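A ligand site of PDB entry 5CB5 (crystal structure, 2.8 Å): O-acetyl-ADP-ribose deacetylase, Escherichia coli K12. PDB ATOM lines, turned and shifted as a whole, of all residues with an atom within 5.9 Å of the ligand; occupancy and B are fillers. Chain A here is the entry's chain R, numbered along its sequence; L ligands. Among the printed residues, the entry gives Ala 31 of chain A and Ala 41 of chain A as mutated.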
ATOM      1  N   GLY A  16      12.080 -28.997  29.128  1.00  0.00           N
ATOM      2  CA  GLY A  16      11.372 -29.588  28.005  1.00  0.00           C
ATOM      3  C   GLY A  16       9.966 -29.101  27.806  1.00  0.00           C
ATOM      4  O   GLY A  16       9.657 -27.928  27.988  1.00  0.00           O
ATOM      5  N   ASP A  17       9.156 -30.031  27.321  1.00  0.00           N
ATOM      6  CA  ASP A  17       7.801 -29.755  26.878  1.00  0.00           C
ATOM      7  C   ASP A  17       6.822 -30.020  28.007  1.00  0.00           C
ATOM      8  O   ASP A  17       6.544 -31.162  28.370  1.00  0.00           O
ATOM      9  CB  ASP A  17       7.428 -30.585  25.622  1.00  0.00           C
ATOM     10  CG  ASP A  17       6.022 -30.269  25.077  1.00  0.00           C
ATOM     11  OD1 ASP A  17       5.367 -29.293  25.518  1.00  0.00           O
ATOM     12  OD2 ASP A  17       5.576 -31.011  24.188  1.00  0.00           O
ATOM     13  N   ILE A  18       6.234 -28.934  28.484  1.00  0.00           N
ATOM     14  CA  ILE A  18       5.238 -28.943  29.602  1.00  0.00           C
ATOM     15  C   ILE A  18       4.065 -29.929  29.399  1.00  0.00           C
ATOM     16  O   ILE A  18       3.507 -30.440  30.340  1.00  0.00           O
ATOM     17  CB  ILE A  18       4.663 -27.546  29.883  1.00  0.00           C
ATOM     18  CG1 ILE A  18       3.928 -27.540  31.228  1.00  0.00           C
ATOM     19  CG2 ILE A  18       3.712 -27.098  28.786  1.00  0.00           C
ATOM     20  CD1 ILE A  18       3.806 -26.154  31.846  1.00  0.00           C
ATOM     21  N   THR A  19       3.686 -30.160  28.157  1.00  0.00           N
ATOM     22  CA  THR A  19       2.512 -31.017  27.822  1.00  0.00           C
ATOM     23  C   THR A  19       2.720 -32.482  28.109  1.00  0.00           C
ATOM     24  O   THR A  19       1.841 -33.323  28.031  1.00  0.00           O
ATOM     25  CB  THR A  19       2.113 -30.904  26.367  1.00  0.00           C
ATOM     26  OG1 THR A  19       3.229 -31.165  25.507  1.00  0.00           O
ATOM     27  CG2 THR A  19       1.588 -29.508  26.081  1.00  0.00           C
ATOM     28  N   ALA A  29      -0.086 -20.359  29.839  1.00  0.00           N
ATOM     29  CA  ALA A  29       0.187 -18.914  29.628  1.00  0.00           C
ATOM     30  C   ALA A  29      -0.786 -18.407  28.557  1.00  0.00           C
ATOM     31  O   ALA A  29      -0.531 -18.450  27.341  1.00  0.00           O
ATOM     32  CB  ALA A  29       1.622 -18.628  29.233  1.00  0.00           C
ATOM     33  N   ALA A  30      -1.888 -17.911  29.066  1.00  0.00           N
ATOM     34  CA  ALA A  30      -3.048 -17.588  28.251  1.00  0.00           C
ATOM     35  C   ALA A  30      -3.215 -16.127  27.972  1.00  0.00           C
ATOM     36  O   ALA A  30      -2.507 -15.256  28.503  1.00  0.00           O
ATOM     37  CB  ALA A  30      -4.316 -18.124  28.884  1.00  0.00           C
ATOM     38  N   ALA A  31      -4.128 -15.874  27.055  1.00  0.00           N
ATOM     39  CA  ALA A  31      -4.652 -14.513  26.758  1.00  0.00           C
ATOM     40  C   ALA A  31      -6.066 -14.374  27.352  1.00  0.00           C
ATOM     41  O   ALA A  31      -6.739 -15.377  27.557  1.00  0.00           O
ATOM     42  CB  ALA A  31      -4.682 -14.256  25.255  1.00  0.00           C
ATOM     43  N   GLY A  36      -6.813 -19.997  22.947  1.00  0.00           N
ATOM     44  CA  GLY A  36      -5.768 -20.694  22.230  1.00  0.00           C
ATOM     45  C   GLY A  36      -4.907 -19.647  21.571  1.00  0.00           C
ATOM     46  O   GLY A  36      -5.307 -18.517  21.374  1.00  0.00           O
ATOM     47  N   GLY A  37      -3.713 -20.064  21.242  1.00  0.00           N
ATOM     48  CA  GLY A  37      -2.709 -19.124  20.750  1.00  0.00           C
ATOM     49  C   GLY A  37      -1.514 -19.795  20.150  1.00  0.00           C
ATOM     50  O   GLY A  37      -1.592 -20.912  19.625  1.00  0.00           O
ATOM     51  N   GLY A  38      -0.390 -19.125  20.250  1.00  0.00           N
ATOM     52  CA  GLY A  38       0.832 -19.637  19.612  1.00  0.00           C
ATOM     53  C   GLY A  38       1.720 -20.496  20.499  1.00  0.00           C
ATOM     54  O   GLY A  38       2.110 -21.605  20.147  1.00  0.00           O
ATOM     55  N   GLY A  39       2.043 -19.982  21.652  1.00  0.00           N
ATOM     56  CA  GLY A  39       3.258 -20.471  22.303  1.00  0.00           C
ATOM     57  C   GLY A  39       3.250 -21.781  23.093  1.00  0.00           C
ATOM     58  O   GLY A  39       3.785 -22.858  22.700  1.00  0.00           O
ATOM     59  N   VAL A  40       2.757 -21.647  24.300  1.00  0.00           N
ATOM     60  CA  VAL A  40       2.441 -22.805  25.130  1.00  0.00           C
ATOM     61  C   VAL A  40       0.973 -23.120  24.920  1.00  0.00           C
ATOM     62  O   VAL A  40       0.549 -24.249  24.788  1.00  0.00           O
ATOM     63  CB  VAL A  40       2.603 -22.589  26.643  1.00  0.00           C
ATOM     64  CG1 VAL A  40       3.161 -23.843  27.271  1.00  0.00           C
ATOM     65  CG2 VAL A  40       3.485 -21.414  26.978  1.00  0.00           C
ATOM     66  N   ALA A  41       0.225 -22.035  24.855  1.00  0.00           N
ATOM     67  CA  ALA A  41      -1.235 -22.101  24.676  1.00  0.00           C
ATOM     68  C   ALA A  41      -1.604 -23.032  23.502  1.00  0.00           C
ATOM     69  O   ALA A  41      -2.509 -23.866  23.601  1.00  0.00           O
ATOM     70  CB  ALA A  41      -1.797 -20.718  24.428  1.00  0.00           C
ATOM     71  N   GLY A  42      -0.866 -22.881  22.413  1.00  0.00           N
ATOM     72  CA  GLY A  42      -1.081 -23.717  21.231  1.00  0.00           C
ATOM     73  C   GLY A  42      -0.674 -25.167  21.510  1.00  0.00           C
ATOM     74  O   GLY A  42      -1.392 -26.132  21.237  1.00  0.00           O
ATOM     75  N   ALA A  43       0.527 -25.302  22.017  1.00  0.00           N
ATOM     76  CA  ALA A  43       1.078 -26.650  22.392  1.00  0.00           C
ATOM     77  C   ALA A  43       0.080 -27.435  23.277  1.00  0.00           C
ATOM     78  O   ALA A  43      -0.271 -28.599  23.036  1.00  0.00           O
ATOM     79  CB  ALA A  43       2.392 -26.500  23.131  1.00  0.00           C
ATOM     80  N   GLY A  89      -0.782 -13.660  32.028  1.00  0.00           N
ATOM     81  CA  GLY A  89       0.390 -12.824  32.327  1.00  0.00           C
ATOM     82  C   GLY A  89       0.260 -11.424  31.750  1.00  0.00           C
ATOM     83  O   GLY A  89      -0.560 -11.167  30.857  1.00  0.00           O
ATOM     84  N   PRO A 125       5.049 -22.851  33.090  1.00  0.00           N
ATOM     85  CA  PRO A 125       5.944 -22.333  32.103  1.00  0.00           C
ATOM     86  C   PRO A 125       6.391 -20.930  32.456  1.00  0.00           C
ATOM     87  O   PRO A 125       5.916 -20.337  33.402  1.00  0.00           O
ATOM     88  CB  PRO A 125       5.064 -22.289  30.848  1.00  0.00           C
ATOM     89  CG  PRO A 125       3.724 -21.963  31.381  1.00  0.00           C
ATOM     90  CD  PRO A 125       3.653 -22.559  32.750  1.00  0.00           C
ATOM     91  N   ALA A 126       7.279 -20.414  31.615  1.00  0.00           N
ATOM     92  CA  ALA A 126       7.847 -19.076  31.811  1.00  0.00           C
ATOM     93  C   ALA A 126       6.893 -18.011  31.339  1.00  0.00           C
ATOM     94  O   ALA A 126       7.010 -17.449  30.237  1.00  0.00           O
ATOM     95  CB  ALA A 126       9.207 -18.936  31.151  1.00  0.00           C
ATOM     96  N   ILE A 127       5.917 -17.760  32.191  1.00  0.00           N
ATOM     97  CA  ILE A 127       4.797 -16.864  31.874  1.00  0.00           C
ATOM     98  C   ILE A 127       5.301 -15.484  31.509  1.00  0.00           C
ATOM     99  O   ILE A 127       6.140 -14.906  32.178  1.00  0.00           O
ATOM    100  CB  ILE A 127       3.774 -16.721  33.023  1.00  0.00           C
ATOM    101  CG1 ILE A 127       3.028 -18.028  33.207  1.00  0.00           C
ATOM    102  CG2 ILE A 127       2.744 -15.633  32.727  1.00  0.00           C
ATOM    103  CD1 ILE A 127       2.383 -18.157  34.564  1.00  0.00           C
ATOM    104  N   SER A 128       4.719 -14.966  30.429  1.00  0.00           N
ATOM    105  CA  SER A 128       4.936 -13.576  29.893  1.00  0.00           C
ATOM    106  C   SER A 128       6.239 -13.330  29.112  1.00  0.00           C
ATOM    107  O   SER A 128       6.453 -12.265  28.535  1.00  0.00           O
ATOM    108  CB  SER A 128       4.799 -12.520  31.004  1.00  0.00           C
ATOM    109  OG  SER A 128       3.445 -12.221  31.264  1.00  0.00           O
ATOM    110  N   THR A 129       7.086 -14.342  29.106  1.00  0.00           N
ATOM    111  CA  THR A 129       8.456 -14.230  28.527  1.00  0.00           C
ATOM    112  C   THR A 129       8.542 -14.506  27.056  1.00  0.00           C
ATOM    113  O   THR A 129       9.568 -14.282  26.427  1.00  0.00           O
ATOM    114  CB  THR A 129       9.479 -15.162  29.185  1.00  0.00           C
ATOM    115  OG1 THR A 129       9.084 -16.525  28.994  1.00  0.00           O
ATOM    116  CG2 THR A 129       9.620 -14.825  30.653  1.00  0.00           C
ATOM    117  N   GLY A 130       7.448 -14.997  26.515  1.00  0.00           N
ATOM    118  CA  GLY A 130       7.384 -15.248  25.069  1.00  0.00           C
ATOM    119  C   GLY A 130       6.886 -14.032  24.290  1.00  0.00           C
ATOM    120  O   GLY A 130       7.548 -12.997  24.202  1.00  0.00           O
ATOM    121  N   VAL A 131       5.717 -14.199  23.702  1.00  0.00           N
ATOM    122  CA  VAL A 131       5.111 -13.154  22.835  1.00  0.00           C
ATOM    123  C   VAL A 131       4.825 -11.875  23.673  1.00  0.00           C
ATOM    124  O   VAL A 131       4.902 -10.768  23.177  1.00  0.00           O
ATOM    125  CB  VAL A 131       3.922 -13.612  21.926  1.00  0.00           C
ATOM    126  CG1 VAL A 131       3.713 -15.117  21.910  1.00  0.00           C
ATOM    127  CG2 VAL A 131       2.665 -12.888  22.327  1.00  0.00           C
ATOM    128  N   TYR A 132       4.549 -12.043  24.963  1.00  0.00           N
ATOM    129  CA  TYR A 132       4.278 -10.897  25.880  1.00  0.00           C
ATOM    130  C   TYR A 132       5.531 -10.087  26.285  1.00  0.00           C
ATOM    131  O   TYR A 132       5.456  -9.058  26.951  1.00  0.00           O
ATOM    132  CB  TYR A 132       3.511 -11.354  27.112  1.00  0.00           C
ATOM    133  CG  TYR A 132       2.020 -11.464  26.896  1.00  0.00           C
ATOM    134  CD1 TYR A 132       1.467 -11.352  25.629  1.00  0.00           C
ATOM    135  CD2 TYR A 132       1.156 -11.716  27.961  1.00  0.00           C
ATOM    136  CE1 TYR A 132       0.089 -11.466  25.437  1.00  0.00           C
ATOM    137  CE2 TYR A 132      -0.212 -11.839  27.771  1.00  0.00           C
ATOM    138  CZ  TYR A 132      -0.746 -11.704  26.506  1.00  0.00           C
ATOM    139  OH  TYR A 132      -2.096 -11.822  26.292  1.00  0.00           O
ATOM    140  N   GLY A 133       6.663 -10.605  25.875  1.00  0.00           N
ATOM    141  CA  GLY A 133       7.961  -9.864  25.838  1.00  0.00           C
ATOM    142  C   GLY A 133       8.573  -9.406  27.143  1.00  0.00           C
ATOM    143  O   GLY A 133       9.228  -8.372  27.202  1.00  0.00           O
ATOM    144  N   VAL A 163       8.799 -25.629  34.374  1.00  0.00           N
ATOM    145  CA  VAL A 163       9.132 -26.131  33.024  1.00  0.00           C
ATOM    146  C   VAL A 163       9.729 -25.058  32.136  1.00  0.00           C
ATOM    147  O   VAL A 163       9.133 -24.036  31.808  1.00  0.00           O
ATOM    148  CB  VAL A 163       7.960 -26.774  32.304  1.00  0.00           C
ATOM    149  CG1 VAL A 163       8.454 -27.466  31.040  1.00  0.00           C
ATOM    150  CG2 VAL A 163       7.322 -27.802  33.213  1.00  0.00           C
ATOM    151  N   CYS A 164      10.950 -25.356  31.739  1.00  0.00           N
ATOM    152  CA  CYS A 164      11.753 -24.463  30.889  1.00  0.00           C
ATOM    153  C   CYS A 164      11.978 -25.059  29.501  1.00  0.00           C
ATOM    154  O   CYS A 164      12.409 -26.210  29.357  1.00  0.00           O
ATOM    155  CB  CYS A 164      13.089 -24.125  31.551  1.00  0.00           C
ATOM    156  SG  CYS A 164      12.846 -23.289  33.131  1.00  0.00           S
ATOM    157  N   TYR A 165      11.725 -24.230  28.495  1.00  0.00           N
ATOM    158  CA  TYR A 165      11.676 -24.694  27.067  1.00  0.00           C
ATOM    159  C   TYR A 165      13.018 -24.785  26.371  1.00  0.00           C
ATOM    160  O   TYR A 165      13.178 -25.438  25.350  1.00  0.00           O
ATOM    161  CB  TYR A 165      10.732 -23.825  26.234  1.00  0.00           C
ATOM    162  CG  TYR A 165      10.217 -24.573  25.017  1.00  0.00           C
ATOM    163  CD1 TYR A 165       9.766 -25.885  25.129  1.00  0.00           C
ATOM    164  CD2 TYR A 165      10.188 -23.984  23.761  1.00  0.00           C
ATOM    165  CE1 TYR A 165       9.309 -26.581  24.038  1.00  0.00           C
ATOM    166  CE2 TYR A 165       9.711 -24.684  22.663  1.00  0.00           C
ATOM    167  CZ  TYR A 165       9.282 -25.974  22.809  1.00  0.00           C
ATOM    168  OH  TYR A 165       8.817 -26.677  21.732  1.00  0.00           O
ATOM    169  N   ASP A 166      13.970 -24.081  26.933  1.00  0.00           N
ATOM    170  CA  ASP A 166      15.355 -24.074  26.457  1.00  0.00           C
ATOM    171  C   ASP A 166      16.351 -24.175  27.626  1.00  0.00           C
ATOM    172  O   ASP A 166      16.006 -23.931  28.770  1.00  0.00           O
ATOM    173  CB  ASP A 166      15.673 -22.857  25.578  1.00  0.00           C
ATOM    174  CG  ASP A 166      15.629 -21.548  26.337  1.00  0.00           C
ATOM    175  OD1 ASP A 166      15.994 -21.524  27.515  1.00  0.00           O
ATOM    176  OD2 ASP A 166      15.268 -20.522  25.730  1.00  0.00           O
ATOM    177  N   ASN A 169      17.312 -20.794  29.704  1.00  0.00           N
ATOM    178  CA  ASN A 169      16.256 -20.488  30.702  1.00  0.00           C
ATOM    179  C   ASN A 169      16.304 -21.441  31.917  1.00  0.00           C
ATOM    180  O   ASN A 169      16.231 -21.046  33.070  1.00  0.00           O
ATOM    181  CB  ASN A 169      14.888 -20.485  30.037  1.00  0.00           C
ATOM    182  CG  ASN A 169      14.195 -19.141  30.206  1.00  0.00           C
ATOM    183  OD1 ASN A 169      14.177 -18.739  31.291  1.00  0.00           O
ATOM    184  ND2 ASN A 169      13.743 -18.420  29.141  1.00  0.00           N
HETATM  185  N1  LIG L   1       6.499 -25.971  27.120  1.00  0.00           N
HETATM  186  C1  LIG L   1       7.027 -25.100  27.998  1.00  0.00           C
HETATM  187  N2  LIG L   1       7.330 -23.858  27.646  1.00  0.00           N
HETATM  188  C2  LIG L   1       7.082 -23.454  26.397  1.00  0.00           C
HETATM  189  C3  LIG L   1       6.525 -24.340  25.401  1.00  0.00           C
HETATM  190  C4  LIG L   1       6.226 -25.680  25.844  1.00  0.00           C
HETATM  191  N3  LIG L   1       5.702 -26.616  25.069  1.00  0.00           N
HETATM  192  N4  LIG L   1       6.419 -23.643  24.255  1.00  0.00           N
HETATM  193  C5  LIG L   1       6.887 -22.388  24.524  1.00  0.00           C
HETATM  194  N5  LIG L   1       7.290 -22.319  25.811  1.00  0.00           N
HETATM  195  C6  LIG L   1       7.802 -21.225  26.562  1.00  0.00           C
HETATM  196  C7  LIG L   1       8.177 -20.026  25.747  1.00  0.00           C
HETATM  197  O1  LIG L   1       9.502 -20.272  25.317  1.00  0.00           O
HETATM  198  C8  LIG L   1       8.148 -18.980  26.823  1.00  0.00           C
HETATM  199  O2  LIG L   1       9.404 -19.074  27.533  1.00  0.00           O
HETATM  200  O3  LIG L   1       6.708 -20.772  27.354  1.00  0.00           O
HETATM  201  C9  LIG L   1       6.991 -19.437  27.738  1.00  0.00           C
HETATM  202  C10 LIG L   1       5.661 -18.722  27.656  1.00  0.00           C
HETATM  203  O4  LIG L   1       5.660 -17.684  26.685  1.00  0.00           O
HETATM  204  P1  LIG L   1       4.416 -17.620  25.649  1.00  0.00           P
HETATM  205  O5  LIG L   1       4.789 -16.874  24.381  1.00  0.00           O
HETATM  206  O6  LIG L   1       3.913 -19.039  25.440  1.00  0.00           O
HETATM  207  O7  LIG L   1       3.215 -16.894  26.442  1.00  0.00           O
HETATM  208  P2  LIG L   1       3.265 -15.420  27.021  1.00  0.00           P
HETATM  209  O8  LIG L   1       2.811 -15.449  28.450  1.00  0.00           O
HETATM  210  O9  LIG L   1       4.594 -14.738  26.842  1.00  0.00           O
HETATM  211  O10 LIG L   1       2.169 -14.636  26.119  1.00  0.00           O
HETATM  212  C11 LIG L   1       1.052 -15.423  25.791  1.00  0.00           C
HETATM  213  O11 LIG L   1       0.997 -15.855  23.416  1.00  0.00           O
HETATM  214  O12 LIG L   1       0.912 -18.165  23.322  1.00  0.00           O
HETATM  215  C12 LIG L   1       0.110 -16.960  23.185  1.00  0.00           C
HETATM  216  O13 LIG L   1      -2.305 -17.092  23.761  1.00  0.00           O
HETATM  217  C13 LIG L   1      -0.986 -16.759  24.228  1.00  0.00           C
HETATM  218  O14 LIG L   1      -1.583 -14.508  23.520  1.00  0.00           O
HETATM  219  C14 LIG L   1      -0.951 -15.267  24.542  1.00  0.00           C
HETATM  220  C15 LIG L   1       0.504 -14.995  24.463  1.00  0.00           C
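N of Ile 18 is in hydrogen-bond range of N1 of the ligand (3.3 Å). The backbone NH of Gly 130 lies within hydrogen-bond range of an oxygen (O9) of the ligand. An oxygen (O5) of the ligand lies within hydrogen-bond range of the backbone NH (N) of Val 131 (2.9 Å). N of Val 40 lies close to O6 of the ligand, at 3.1 Å. N of Tyr 132 lies within hydrogen-bond range of O9 of the ligand (3.3 Å). An oxygen (O9) of the ligand lies within hydrogen-bond range of the backbone NH (N) of Thr 129 (3.4 Å). N3 of the ligand lies within hydrogen-bond range of OD1 of Asp 17, 2.7 Å away. The backbone NH of Gly 38 is in hydrogen-bond range of an oxygen (O12) of the ligand. The backbone NH of Ser 128 sits at hydrogen-bond distance from an oxygen (O8) of the ligand (2.8 Å). The side-chain hydroxyl (OG1) of Thr 129 lies within hydrogen-bond range of an oxygen (O2) of the ligand. An oxygen (O12) of the ligand sits at hydrogen-bond distance from the backbone NH (N) of Gly 39, 2.7 Å away.
The backbone carbonyl oxygen (O) of Cys 164 lies within hydrogen-bond range of the backbone NH (N) of Gly 16, at 2.8 Å. O of Ser 128 sits at hydrogen-bond distance from N of Gly 133 (3.1 Å). OG1 of Thr 129 sits at hydrogen-bond distance from O of Ala 126 (2.6 Å). OD2 of Asp 17 sits at hydrogen-bond distance from OG1 of Thr 19. The backbone NH (N) of Gly 42 sits close to the backbone carbonyl oxygen (O) of Gly 37, 3.5 Å away.
Gly 16 touches the ligand (O to N1, 3.8 Å). Ala 29 touches the ligand (CB to O8, 3.5 Å). CB of Ala 31 touches O14 of the ligand (3.6 Å). CA of Gly 37 touches O13 of the ligand (3.7 Å). Ala 41 touches the ligand. CB of Ala 43 touches N3 of the ligand (3.8 Å). O of Ala 126 touches C10 of the ligand, 3.2 Å away. C of Ile 127 touches O8 of the ligand, 3.9 Å away. Tyr 165 touches the ligand. 19 residues have an atom within 4 Å of the ligand: Gly 16, Asp 17, Ile 18, Ala 29, Ala 31, Gly 37, Gly 38, Gly 39, Val 40, Ala 41, Ala 43, Ala 126, Ile 127, Ser 128, Thr 129, Gly 130, Val 131, Tyr 132 and Tyr 165. Along chain A the residues within 4 Å of the ligand span positions 16 to 165.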
